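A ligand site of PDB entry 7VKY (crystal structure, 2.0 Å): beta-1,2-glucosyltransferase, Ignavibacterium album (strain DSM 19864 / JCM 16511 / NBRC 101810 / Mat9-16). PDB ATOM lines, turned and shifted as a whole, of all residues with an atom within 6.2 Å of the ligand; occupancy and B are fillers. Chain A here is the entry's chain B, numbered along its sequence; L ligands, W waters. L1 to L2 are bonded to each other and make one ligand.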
ATOM      1  N   HIS A  20       7.207  15.620  20.225  1.00  0.00           N
ATOM      2  CA  HIS A  20       6.981  14.210  19.839  1.00  0.00           C
ATOM      3  C   HIS A  20       6.008  13.604  20.841  1.00  0.00           C
ATOM      4  O   HIS A  20       6.453  13.142  21.931  1.00  0.00           O
ATOM      5  CB  HIS A  20       8.293  13.455  19.699  1.00  0.00           C
ATOM      6  CG  HIS A  20       9.157  13.876  18.546  1.00  0.00           C
ATOM      7  ND1 HIS A  20      10.456  13.407  18.401  1.00  0.00           N
ATOM      8  CD2 HIS A  20       8.942  14.723  17.511  1.00  0.00           C
ATOM      9  CE1 HIS A  20      10.983  13.916  17.309  1.00  0.00           C
ATOM     10  NE2 HIS A  20      10.097  14.761  16.765  1.00  0.00           N
ATOM     11  N   TYR A  47       6.887  13.858  14.024  1.00  0.00           N
ATOM     12  CA  TYR A  47       6.841  12.582  13.289  1.00  0.00           C
ATOM     13  C   TYR A  47       5.563  11.843  13.704  1.00  0.00           C
ATOM     14  O   TYR A  47       5.051  12.102  14.829  1.00  0.00           O
ATOM     15  CB  TYR A  47       8.122  11.797  13.513  1.00  0.00           C
ATOM     16  CG  TYR A  47       9.368  12.490  12.999  1.00  0.00           C
ATOM     17  CD1 TYR A  47       9.579  12.696  11.637  1.00  0.00           C
ATOM     18  CD2 TYR A  47      10.350  12.924  13.871  1.00  0.00           C
ATOM     19  CE1 TYR A  47      10.750  13.265  11.177  1.00  0.00           C
ATOM     20  CE2 TYR A  47      11.493  13.534  13.411  1.00  0.00           C
ATOM     21  CZ  TYR A  47      11.715  13.693  12.066  1.00  0.00           C
ATOM     22  OH  TYR A  47      12.887  14.258  11.666  1.00  0.00           O
ATOM     23  N   ILE A  94      11.916   8.328   9.513  1.00  0.00           N
ATOM     24  CA  ILE A  94      11.874   9.541  10.373  1.00  0.00           C
ATOM     25  C   ILE A  94      13.262   9.853  10.947  1.00  0.00           C
ATOM     26  O   ILE A  94      13.492  10.987  11.356  1.00  0.00           O
ATOM     27  CB  ILE A  94      10.807   9.396  11.458  1.00  0.00           C
ATOM     28  CG1 ILE A  94      11.192   8.399  12.566  1.00  0.00           C
ATOM     29  CG2 ILE A  94       9.470   9.035  10.855  1.00  0.00           C
ATOM     30  CD1 ILE A  94      10.321   8.539  13.787  1.00  0.00           C
ATOM     31  N   LEU A  95      14.155   8.858  11.000  1.00  0.00           N
ATOM     32  CA  LEU A  95      15.459   8.947  11.726  1.00  0.00           C
ATOM     33  C   LEU A  95      15.192   9.253  13.196  1.00  0.00           C
ATOM     34  O   LEU A  95      14.822   8.300  13.930  1.00  0.00           O
ATOM     35  CB  LEU A  95      16.381   9.967  11.041  1.00  0.00           C
ATOM     36  CG  LEU A  95      17.183   9.409   9.868  1.00  0.00           C
ATOM     37  CD1 LEU A  95      16.280   9.033   8.693  1.00  0.00           C
ATOM     38  CD2 LEU A  95      18.271  10.394   9.454  1.00  0.00           C
ATOM     39  N   ALA A  96      15.322  10.521  13.613  1.00  0.00           N
ATOM     40  CA  ALA A  96      14.861  11.043  14.927  1.00  0.00           C
ATOM     41  C   ALA A  96      15.400  10.177  16.086  1.00  0.00           C
ATOM     42  O   ALA A  96      14.749  10.155  17.156  1.00  0.00           O
ATOM     43  CB  ALA A  96      13.354  11.084  14.946  1.00  0.00           C
ATOM     44  N   GLU A  97      16.578   9.538  15.906  1.00  0.00           N
ATOM     45  CA  GLU A  97      17.250   8.713  16.944  1.00  0.00           C
ATOM     46  C   GLU A  97      16.244   7.690  17.477  1.00  0.00           C
ATOM     47  O   GLU A  97      16.241   7.412  18.682  1.00  0.00           O
ATOM     48  CB  GLU A  97      17.800   9.630  18.051  1.00  0.00           C
ATOM     49  CG  GLU A  97      19.054  10.412  17.652  1.00  0.00           C
ATOM     50  CD  GLU A  97      18.863  11.608  16.726  1.00  0.00           C
ATOM     51  OE1 GLU A  97      19.527  11.645  15.644  1.00  0.00           O
ATOM     52  OE2 GLU A  97      18.047  12.524  17.060  1.00  0.00           O
ATOM     53  N   GLN A 167       5.782  16.556   5.717  1.00  0.00           N
ATOM     54  CA  GLN A 167       7.086  16.157   5.172  1.00  0.00           C
ATOM     55  C   GLN A 167       7.011  14.741   4.578  1.00  0.00           C
ATOM     56  O   GLN A 167       6.428  13.858   5.217  1.00  0.00           O
ATOM     57  CB  GLN A 167       8.129  16.294   6.272  1.00  0.00           C
ATOM     58  CG  GLN A 167       9.545  16.054   5.791  1.00  0.00           C
ATOM     59  CD  GLN A 167      10.487  16.118   6.967  1.00  0.00           C
ATOM     60  OE1 GLN A 167      10.837  17.190   7.458  1.00  0.00           O
ATOM     61  NE2 GLN A 167      10.867  14.949   7.446  1.00  0.00           N
ATOM     62  N   ASN A 170      12.280  11.529   5.260  1.00  0.00           N
ATOM     63  CA  ASN A 170      13.225  12.297   6.084  1.00  0.00           C
ATOM     64  C   ASN A 170      14.618  12.212   5.448  1.00  0.00           C
ATOM     65  O   ASN A 170      15.156  11.090   5.290  1.00  0.00           O
ATOM     66  CB  ASN A 170      13.215  11.788   7.530  1.00  0.00           C
ATOM     67  CG  ASN A 170      13.828  12.790   8.484  1.00  0.00           C
ATOM     68  OD1 ASN A 170      13.159  13.728   8.909  1.00  0.00           O
ATOM     69  ND2 ASN A 170      15.083  12.594   8.819  1.00  0.00           N
ATOM     70  N   GLU A 171      15.154  13.378   5.111  1.00  0.00           N
ATOM     71  CA  GLU A 171      16.550  13.607   4.657  1.00  0.00           C
ATOM     72  C   GLU A 171      16.910  12.503   3.671  1.00  0.00           C
ATOM     73  O   GLU A 171      17.862  11.766   3.924  1.00  0.00           O
ATOM     74  CB  GLU A 171      17.475  13.689   5.871  1.00  0.00           C
ATOM     75  CG  GLU A 171      17.207  14.903   6.759  1.00  0.00           C
ATOM     76  CD  GLU A 171      18.110  15.015   7.992  1.00  0.00           C
ATOM     77  OE1 GLU A 171      18.529  13.977   8.455  1.00  0.00           O
ATOM     78  OE2 GLU A 171      18.441  16.178   8.435  1.00  0.00           O
ATOM     79  N   VAL A 174      20.462  10.489   3.186  1.00  0.00           N
ATOM     80  CA  VAL A 174      21.309  10.761   4.381  1.00  0.00           C
ATOM     81  C   VAL A 174      22.162   9.530   4.770  1.00  0.00           C
ATOM     82  O   VAL A 174      23.195   9.764   5.409  1.00  0.00           O
ATOM     83  CB  VAL A 174      20.466  11.281   5.565  1.00  0.00           C
ATOM     84  CG1 VAL A 174      19.660  10.177   6.234  1.00  0.00           C
ATOM     85  CG2 VAL A 174      21.307  12.038   6.593  1.00  0.00           C
ATOM     86  N   TRP A 177      25.090   9.111   2.471  1.00  0.00           N
ATOM     87  CA  TRP A 177      26.056  10.141   2.910  1.00  0.00           C
ATOM     88  C   TRP A 177      26.831   9.625   4.122  1.00  0.00           C
ATOM     89  O   TRP A 177      28.065   9.518   3.999  1.00  0.00           O
ATOM     90  CB  TRP A 177      25.342  11.457   3.202  1.00  0.00           C
ATOM     91  CG  TRP A 177      26.226  12.473   3.847  1.00  0.00           C
ATOM     92  CD1 TRP A 177      27.487  12.846   3.494  1.00  0.00           C
ATOM     93  CD2 TRP A 177      25.869  13.269   4.988  1.00  0.00           C
ATOM     94  NE1 TRP A 177      27.955  13.792   4.369  1.00  0.00           N
ATOM     95  CE2 TRP A 177      26.967  14.104   5.270  1.00  0.00           C
ATOM     96  CE3 TRP A 177      24.712  13.358   5.773  1.00  0.00           C
ATOM     97  CZ2 TRP A 177      26.959  15.010   6.319  1.00  0.00           C
ATOM     98  CZ3 TRP A 177      24.710  14.243   6.818  1.00  0.00           C
ATOM     99  CH2 TRP A 177      25.808  15.053   7.079  1.00  0.00           C
ATOM    100  N   LEU A 178      26.154   9.295   5.223  1.00  0.00           N
ATOM    101  CA  LEU A 178      26.784   8.955   6.521  1.00  0.00           C
ATOM    102  C   LEU A 178      27.762   7.753   6.370  1.00  0.00           C
ATOM    103  O   LEU A 178      28.751   7.715   7.104  1.00  0.00           O
ATOM    104  CB  LEU A 178      25.696   8.702   7.564  1.00  0.00           C
ATOM    105  CG  LEU A 178      24.894   9.915   8.054  1.00  0.00           C
ATOM    106  CD1 LEU A 178      23.802   9.490   9.008  1.00  0.00           C
ATOM    107  CD2 LEU A 178      25.759  10.956   8.742  1.00  0.00           C
ATOM    108  N   ASN A 270      13.505  17.964   4.124  1.00  0.00           N
ATOM    109  CA  ASN A 270      14.462  18.579   5.074  1.00  0.00           C
ATOM    110  C   ASN A 270      15.889  18.257   4.658  1.00  0.00           C
ATOM    111  O   ASN A 270      16.152  17.104   4.293  1.00  0.00           O
ATOM    112  CB  ASN A 270      14.110  18.160   6.504  1.00  0.00           C
ATOM    113  CG  ASN A 270      13.989  16.673   6.697  1.00  0.00           C
ATOM    114  OD1 ASN A 270      13.745  15.898   5.751  1.00  0.00           O
ATOM    115  ND2 ASN A 270      14.176  16.263   7.941  1.00  0.00           N
ATOM    116  N   ILE A 271      16.767  19.240   4.735  1.00  0.00           N
ATOM    117  CA  ILE A 271      18.150  19.111   4.207  1.00  0.00           C
ATOM    118  C   ILE A 271      19.131  18.904   5.366  1.00  0.00           C
ATOM    119  O   ILE A 271      19.289  19.763   6.216  1.00  0.00           O
ATOM    120  CB  ILE A 271      18.522  20.356   3.397  1.00  0.00           C
ATOM    121  CG1 ILE A 271      17.531  20.631   2.266  1.00  0.00           C
ATOM    122  CG2 ILE A 271      19.937  20.190   2.885  1.00  0.00           C
ATOM    123  CD1 ILE A 271      17.479  22.088   1.851  1.00  0.00           C
ATOM    124  N   PRO A 272      19.859  17.774   5.402  1.00  0.00           N
ATOM    125  CA  PRO A 272      20.915  17.556   6.385  1.00  0.00           C
ATOM    126  C   PRO A 272      22.239  18.203   5.943  1.00  0.00           C
ATOM    127  O   PRO A 272      22.342  18.665   4.795  1.00  0.00           O
ATOM    128  CB  PRO A 272      21.069  16.015   6.346  1.00  0.00           C
ATOM    129  CG  PRO A 272      20.804  15.650   4.917  1.00  0.00           C
ATOM    130  CD  PRO A 272      19.763  16.660   4.434  1.00  0.00           C
ATOM    131  N   GLY A 273      23.234  18.164   6.809  1.00  0.00           N
ATOM    132  CA  GLY A 273      24.632  18.393   6.408  1.00  0.00           C
ATOM    133  C   GLY A 273      25.480  19.081   7.446  1.00  0.00           C
ATOM    134  O   GLY A 273      26.739  19.137   7.239  1.00  0.00           O
ATOM    135  N   TRP A 274      24.885  19.616   8.502  1.00  0.00           N
ATOM    136  CA  TRP A 274      25.698  20.119   9.630  1.00  0.00           C
ATOM    137  C   TRP A 274      26.329  18.909  10.328  1.00  0.00           C
ATOM    138  O   TRP A 274      25.650  17.864  10.470  1.00  0.00           O
ATOM    139  CB  TRP A 274      24.872  20.926  10.608  1.00  0.00           C
ATOM    140  CG  TRP A 274      24.424  22.277  10.146  1.00  0.00           C
ATOM    141  CD1 TRP A 274      23.446  22.533   9.226  1.00  0.00           C
ATOM    142  CD2 TRP A 274      24.894  23.558  10.599  1.00  0.00           C
ATOM    143  NE1 TRP A 274      23.234  23.876   9.128  1.00  0.00           N
ATOM    144  CE2 TRP A 274      24.096  24.536   9.961  1.00  0.00           C
ATOM    145  CE3 TRP A 274      25.874  23.976  11.510  1.00  0.00           C
ATOM    146  CZ2 TRP A 274      24.309  25.899  10.134  1.00  0.00           C
ATOM    147  CZ3 TRP A 274      26.065  25.328  11.722  1.00  0.00           C
ATOM    148  CH2 TRP A 274      25.276  26.272  11.045  1.00  0.00           C
ATOM    149  N   ILE A 275      27.578  19.046  10.739  1.00  0.00           N
ATOM    150  CA  ILE A 275      28.216  18.079  11.666  1.00  0.00           C
ATOM    151  C   ILE A 275      29.297  18.827  12.451  1.00  0.00           C
ATOM    152  O   ILE A 275      29.915  19.704  11.894  1.00  0.00           O
ATOM    153  CB  ILE A 275      28.701  16.821  10.910  1.00  0.00           C
ATOM    154  CG1 ILE A 275      29.111  15.713  11.878  1.00  0.00           C
ATOM    155  CG2 ILE A 275      29.793  17.167   9.903  1.00  0.00           C
ATOM    156  CD1 ILE A 275      28.940  14.308  11.338  1.00  0.00           C
ATOM    157  N   TYR A 276      29.404  18.576  13.756  1.00  0.00           N
ATOM    158  CA  TYR A 276      30.368  19.256  14.655  1.00  0.00           C
ATOM    159  C   TYR A 276      30.212  20.777  14.559  1.00  0.00           C
ATOM    160  O   TYR A 276      31.178  21.456  14.799  1.00  0.00           O
ATOM    161  CB  TYR A 276      31.810  18.833  14.332  1.00  0.00           C
ATOM    162  CG  TYR A 276      31.984  17.337  14.190  1.00  0.00           C
ATOM    163  CD1 TYR A 276      31.466  16.447  15.128  1.00  0.00           C
ATOM    164  CD2 TYR A 276      32.664  16.807  13.105  1.00  0.00           C
ATOM    165  CE1 TYR A 276      31.579  15.072  14.980  1.00  0.00           C
ATOM    166  CE2 TYR A 276      32.796  15.431  12.934  1.00  0.00           C
ATOM    167  CZ  TYR A 276      32.270  14.570  13.881  1.00  0.00           C
ATOM    168  OH  TYR A 276      32.419  13.221  13.683  1.00  0.00           O
ATOM    169  N   ASP A 304      18.057  21.943   8.037  1.00  0.00           N
ATOM    170  CA  ASP A 304      18.257  21.362   9.381  1.00  0.00           C
ATOM    171  C   ASP A 304      19.533  22.001   9.909  1.00  0.00           C
ATOM    172  O   ASP A 304      20.609  21.476   9.603  1.00  0.00           O
ATOM    173  CB  ASP A 304      18.248  19.832   9.340  1.00  0.00           C
ATOM    174  CG  ASP A 304      16.932  19.259   8.804  1.00  0.00           C
ATOM    175  OD1 ASP A 304      15.937  20.014   8.753  1.00  0.00           O
ATOM    176  OD2 ASP A 304      16.943  18.085   8.430  1.00  0.00           O
ATOM    177  N   ILE A 306      22.130  22.848  12.767  1.00  0.00           N
ATOM    178  CA  ILE A 306      22.672  22.308  14.038  1.00  0.00           C
ATOM    179  C   ILE A 306      24.002  22.991  14.339  1.00  0.00           C
ATOM    180  O   ILE A 306      25.051  22.381  14.206  1.00  0.00           O
ATOM    181  CB  ILE A 306      22.806  20.778  13.990  1.00  0.00           C
ATOM    182  CG1 ILE A 306      21.647  20.118  13.235  1.00  0.00           C
ATOM    183  CG2 ILE A 306      22.980  20.238  15.388  1.00  0.00           C
ATOM    184  CD1 ILE A 306      21.791  18.607  13.060  1.00  0.00           C
ATOM    185  N   GLU A 308      25.359  24.047  17.232  1.00  0.00           N
ATOM    186  CA  GLU A 308      25.953  23.538  18.526  1.00  0.00           C
ATOM    187  C   GLU A 308      26.528  24.679  19.376  1.00  0.00           C
ATOM    188  O   GLU A 308      26.463  24.621  20.656  1.00  0.00           O
ATOM    189  CB  GLU A 308      27.022  22.484  18.295  1.00  0.00           C
ATOM    190  CG  GLU A 308      26.537  21.281  17.494  1.00  0.00           C
ATOM    191  CD  GLU A 308      27.519  20.157  17.238  1.00  0.00           C
ATOM    192  OE1 GLU A 308      28.729  20.307  17.572  1.00  0.00           O
ATOM    193  OE2 GLU A 308      27.072  19.132  16.698  1.00  0.00           O
ATOM    194  N   GLU A 338      14.240  21.946  10.751  1.00  0.00           N
ATOM    195  CA  GLU A 338      14.827  21.606  12.078  1.00  0.00           C
ATOM    196  C   GLU A 338      15.791  22.725  12.485  1.00  0.00           C
ATOM    197  O   GLU A 338      16.821  22.924  11.804  1.00  0.00           O
ATOM    198  CB  GLU A 338      15.542  20.243  12.012  1.00  0.00           C
ATOM    199  CG  GLU A 338      14.603  19.112  11.602  1.00  0.00           C
ATOM    200  CD  GLU A 338      15.266  17.764  11.377  1.00  0.00           C
ATOM    201  OE1 GLU A 338      16.419  17.605  11.799  1.00  0.00           O
ATOM    202  OE2 GLU A 338      14.618  16.893  10.761  1.00  0.00           O
ATOM    203  N   ARG A 344      20.879  17.131  20.691  1.00  0.00           N
ATOM    204  CA  ARG A 344      20.626  15.680  20.489  1.00  0.00           C
ATOM    205  C   ARG A 344      21.555  14.816  21.370  1.00  0.00           C
ATOM    206  O   ARG A 344      21.266  13.630  21.537  1.00  0.00           O
ATOM    207  CB  ARG A 344      20.817  15.335  19.010  1.00  0.00           C
ATOM    208  CG  ARG A 344      22.216  15.581  18.479  1.00  0.00           C
ATOM    209  CD  ARG A 344      22.197  15.768  16.957  1.00  0.00           C
ATOM    210  NE  ARG A 344      23.533  16.030  16.386  1.00  0.00           N
ATOM    211  CZ  ARG A 344      23.898  15.725  15.150  1.00  0.00           C
ATOM    212  NH1 ARG A 344      23.038  15.126  14.342  1.00  0.00           N
ATOM    213  NH2 ARG A 344      25.124  15.964  14.745  1.00  0.00           N
ATOM    214  N   TYR A 373      13.763  22.507  17.043  1.00  0.00           N
ATOM    215  CA  TYR A 373      14.022  21.047  17.095  1.00  0.00           C
ATOM    216  C   TYR A 373      15.196  20.883  18.057  1.00  0.00           C
ATOM    217  O   TYR A 373      16.322  21.167  17.639  1.00  0.00           O
ATOM    218  CB  TYR A 373      14.274  20.550  15.663  1.00  0.00           C
ATOM    219  CG  TYR A 373      14.264  19.055  15.519  1.00  0.00           C
ATOM    220  CD1 TYR A 373      15.284  18.269  16.024  1.00  0.00           C
ATOM    221  CD2 TYR A 373      13.178  18.395  14.951  1.00  0.00           C
ATOM    222  CE1 TYR A 373      15.274  16.888  15.922  1.00  0.00           C
ATOM    223  CE2 TYR A 373      13.151  17.017  14.834  1.00  0.00           C
ATOM    224  CZ  TYR A 373      14.208  16.253  15.313  1.00  0.00           C
ATOM    225  OH  TYR A 373      14.175  14.890  15.207  1.00  0.00           O
ATOM    226  N   MET A 374      14.949  20.489  19.334  1.00  0.00           N
ATOM    227  CA  MET A 374      13.650  20.067  19.875  1.00  0.00           C
ATOM    228  C   MET A 374      13.113  21.092  20.848  1.00  0.00           C
ATOM    229  O   MET A 374      13.811  21.496  21.775  1.00  0.00           O
ATOM    230  CB  MET A 374      13.728  18.724  20.614  1.00  0.00           C
ATOM    231  CG  MET A 374      13.946  17.511  19.715  1.00  0.00           C
ATOM    232  SD  MET A 374      12.631  17.195  18.522  1.00  0.00           S
ATOM    233  CE  MET A 374      11.288  16.886  19.673  1.00  0.00           C
ATOM    234  N   PHE A 391      15.450  11.670  24.886  1.00  0.00           N
ATOM    235  CA  PHE A 391      15.561  12.244  23.516  1.00  0.00           C
ATOM    236  C   PHE A 391      15.739  13.758  23.661  1.00  0.00           C
ATOM    237  O   PHE A 391      14.792  14.441  24.075  1.00  0.00           O
ATOM    238  CB  PHE A 391      14.355  11.883  22.667  1.00  0.00           C
ATOM    239  CG  PHE A 391      14.400  12.485  21.292  1.00  0.00           C
ATOM    240  CD1 PHE A 391      15.399  12.107  20.417  1.00  0.00           C
ATOM    241  CD2 PHE A 391      13.546  13.506  20.939  1.00  0.00           C
ATOM    242  CE1 PHE A 391      15.491  12.682  19.161  1.00  0.00           C
ATOM    243  CE2 PHE A 391      13.611  14.062  19.675  1.00  0.00           C
ATOM    244  CZ  PHE A 391      14.615  13.687  18.817  1.00  0.00           C
ATOM    245  N   TYR A 392      16.941  14.233  23.366  1.00  0.00           N
ATOM    246  CA  TYR A 392      17.381  15.646  23.513  1.00  0.00           C
ATOM    247  C   TYR A 392      17.483  16.091  24.971  1.00  0.00           C
ATOM    248  O   TYR A 392      16.886  15.495  25.909  1.00  0.00           O
ATOM    249  CB  TYR A 392      16.499  16.621  22.722  1.00  0.00           C
ATOM    250  CG  TYR A 392      16.982  16.829  21.318  1.00  0.00           C
ATOM    251  CD1 TYR A 392      16.962  15.802  20.400  1.00  0.00           C
ATOM    252  CD2 TYR A 392      17.399  18.076  20.889  1.00  0.00           C
ATOM    253  CE1 TYR A 392      17.399  15.992  19.103  1.00  0.00           C
ATOM    254  CE2 TYR A 392      17.863  18.284  19.600  1.00  0.00           C
ATOM    255  CZ  TYR A 392      17.850  17.232  18.703  1.00  0.00           C
ATOM    256  OH  TYR A 392      18.254  17.443  17.428  1.00  0.00           O
ATOM    257  N   LEU A 451      32.584  12.628   5.227  1.00  0.00           N
ATOM    258  CA  LEU A 451      32.107  11.400   5.934  1.00  0.00           C
ATOM    259  C   LEU A 451      32.614  10.133   5.240  1.00  0.00           C
ATOM    260  O   LEU A 451      32.935   9.194   5.961  1.00  0.00           O
ATOM    261  CB  LEU A 451      30.580  11.417   6.047  1.00  0.00           C
ATOM    262  CG  LEU A 451      30.087  12.061   7.336  1.00  0.00           C
ATOM    263  CD1 LEU A 451      30.332  13.553   7.333  1.00  0.00           C
ATOM    264  CD2 LEU A 451      28.637  11.757   7.557  1.00  0.00           C
HETATM  265  C1  LIG L   1      21.492  13.629  11.516  1.00  0.00           C
HETATM  266  C2  LIG L   1      20.713  14.915  11.254  1.00  0.00           C
HETATM  267  C3  LIG L   1      21.396  15.693  10.117  1.00  0.00           C
HETATM  268  C4  LIG L   1      22.912  15.865  10.367  1.00  0.00           C
HETATM  269  C5  LIG L   1      23.585  14.499  10.658  1.00  0.00           C
HETATM  270  C6  LIG L   1      25.088  14.621  10.969  1.00  0.00           C
HETATM  271  O1  LIG L   1      21.264  12.888  10.300  1.00  0.00           O
HETATM  272  O2  LIG L   1      19.344  14.504  10.880  1.00  0.00           O
HETATM  273  O3  LIG L   1      20.747  16.975   9.974  1.00  0.00           O
HETATM  274  O4  LIG L   1      23.567  16.548   9.290  1.00  0.00           O
HETATM  275  O5  LIG L   1      22.883  13.902  11.769  1.00  0.00           O
HETATM  276  O6  LIG L   1      25.332  15.539  12.059  1.00  0.00           O
HETATM  277  C1  LG2 L   2      16.967  14.446  11.356  1.00  0.00           C
HETATM  278  C2  LG2 L   2      16.259  14.350  12.709  1.00  0.00           C
HETATM  279  C3  LG2 L   2      17.248  14.223  13.869  1.00  0.00           C
HETATM  280  C4  LG2 L   2      18.069  15.515  13.938  1.00  0.00           C
HETATM  281  C5  LG2 L   2      19.210  15.451  14.975  1.00  0.00           C
HETATM  282  C6  LG2 L   2      18.249  15.327  11.375  1.00  0.00           C
HETATM  283  O1  LG2 L   2      16.034  14.730  10.299  1.00  0.00           O
HETATM  284  O2  LG2 L   2      15.437  13.172  12.681  1.00  0.00           O
HETATM  285  O3  LG2 L   2      16.551  14.002  15.095  1.00  0.00           O
HETATM  286  O4  LG2 L   2      18.647  15.872  12.653  1.00  0.00           O
HETATM  287  O5  LG2 L   2      20.019  14.244  14.821  1.00  0.00           O
HETATM  288  O   HOH W   1      22.182  19.364   9.521  1.00  0.00           O
HETATM  289  O   HOH W   2      18.430  18.892  12.924  1.00  0.00           O
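The side-chain amide nitrogen (ND2) of Asn 270 lies within hydrogen-bond range of the side-chain carboxylate (OD2) of Asp 304 (3.3 Å).
The backbone carbonyl oxygen (O) of Ile 271 sits at hydrogen-bond distance from the backbone NH (N) of Asp 304 (3.1 Å).
OD2 of Asp 304 sits close to OE2 of Glu 171, 2.4 Å away.
The side-chain amide nitrogen (NE2) of Gln 167 lies within hydrogen-bond range of the side-chain amide oxygen (OD1) of Asn 170.
The side-chain amide nitrogen (ND2) of Asn 270 is in hydrogen-bond range of the side-chain carboxylate (OE2) of Glu 338 (2.9 Å).
The side-chain amide nitrogen (ND2) of Asn 170 is in hydrogen-bond range of the backbone carbonyl oxygen (O) of Ile 94.
OE2 of Glu 338 lies within hydrogen-bond range of OH of Tyr 47 (3.3 Å).
The backbone NH (N) of Glu 338 is in hydrogen-bond range of the side-chain carboxylate (OD1) of Asp 304.
Water W1 lies within hydrogen-bond range of O of Asp 304, O3 of LIG L1, N of Trp 274 and N of Gly 273.
Water W2 bridges OE1 of Glu 338 and O4 of LG2 L2.
An oxygen (O1) of LG2 L2 is in hydrogen-bond range of the side-chain amide nitrogen of Asn 170 (2.8 Å).
The guanidinium group of Arg 344 is in hydrogen-bond range of an oxygen (O6) of LIG L1, at 2.7 Å.
An oxygen (O3) of LIG L1 is in hydrogen-bond range of the side-chain carboxylate (OE2) of Glu 171.
The side-chain hydroxyl of Tyr 47 lies within hydrogen-bond range of an oxygen (O2) of LG2 L2.
O5 of LG2 L2 is in hydrogen-bond range of OE1 of Glu 97, 2.8 Å away.
O4 of LIG L1 is in hydrogen-bond range of O of Trp 274.
The side-chain hydroxyl (OH) of Tyr 373 lies within hydrogen-bond range of an oxygen (O3) of LG2 L2 (2.5 Å).
The backbone NH of Ala 96 lies within hydrogen-bond range of an oxygen (O2) of LG2 L2 (2.8 Å).
ND2 of Asn 270 sits at hydrogen-bond distance from O1 of LG2 L2, at 3.4 Å.
O4 of LIG L1 sits at hydrogen-bond distance from N of Gly 273 (3.0 Å).
O1 of LG2 L2 is in hydrogen-bond range of OE2 of Glu 338 (2.6 Å).
The backbone carbonyl oxygen (O) of Ile 94 sits at hydrogen-bond distance from an oxygen (O2) of LG2 L2 (3.2 Å).
The backbone NH of Trp 274 sits at hydrogen-bond distance from an oxygen (O4) of LIG L1, 3.4 Å away.
CB of Leu 95 touches O2 of LG2 L2 (3.7 Å).
Val 174 touches the ligand.
CH2 of Trp 177 touches O4 of LIG L1, at 3.5 Å.
CA of Pro 272 touches O3 of LIG L1 (3.6 Å).
CB of Ile 275 touches O6 of LIG L1, 3.8 Å away.
CB of Asp 304 touches O3 of LIG L1 (3.8 Å).
Ile 306 touches the ligand.
Tyr 392 touches the ligand.
Within 4 Å of the ligand: Tyr 47, Ile 94, Leu 95, Ala 96, Glu 97, Asn 170, Glu 171, Val 174, Trp 177, Asn 270, Pro 272, Gly 273, Trp 274, Ile 275, Asp 304, Ile 306, Glu 338, Arg 344, Tyr 373 and Tyr 392.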
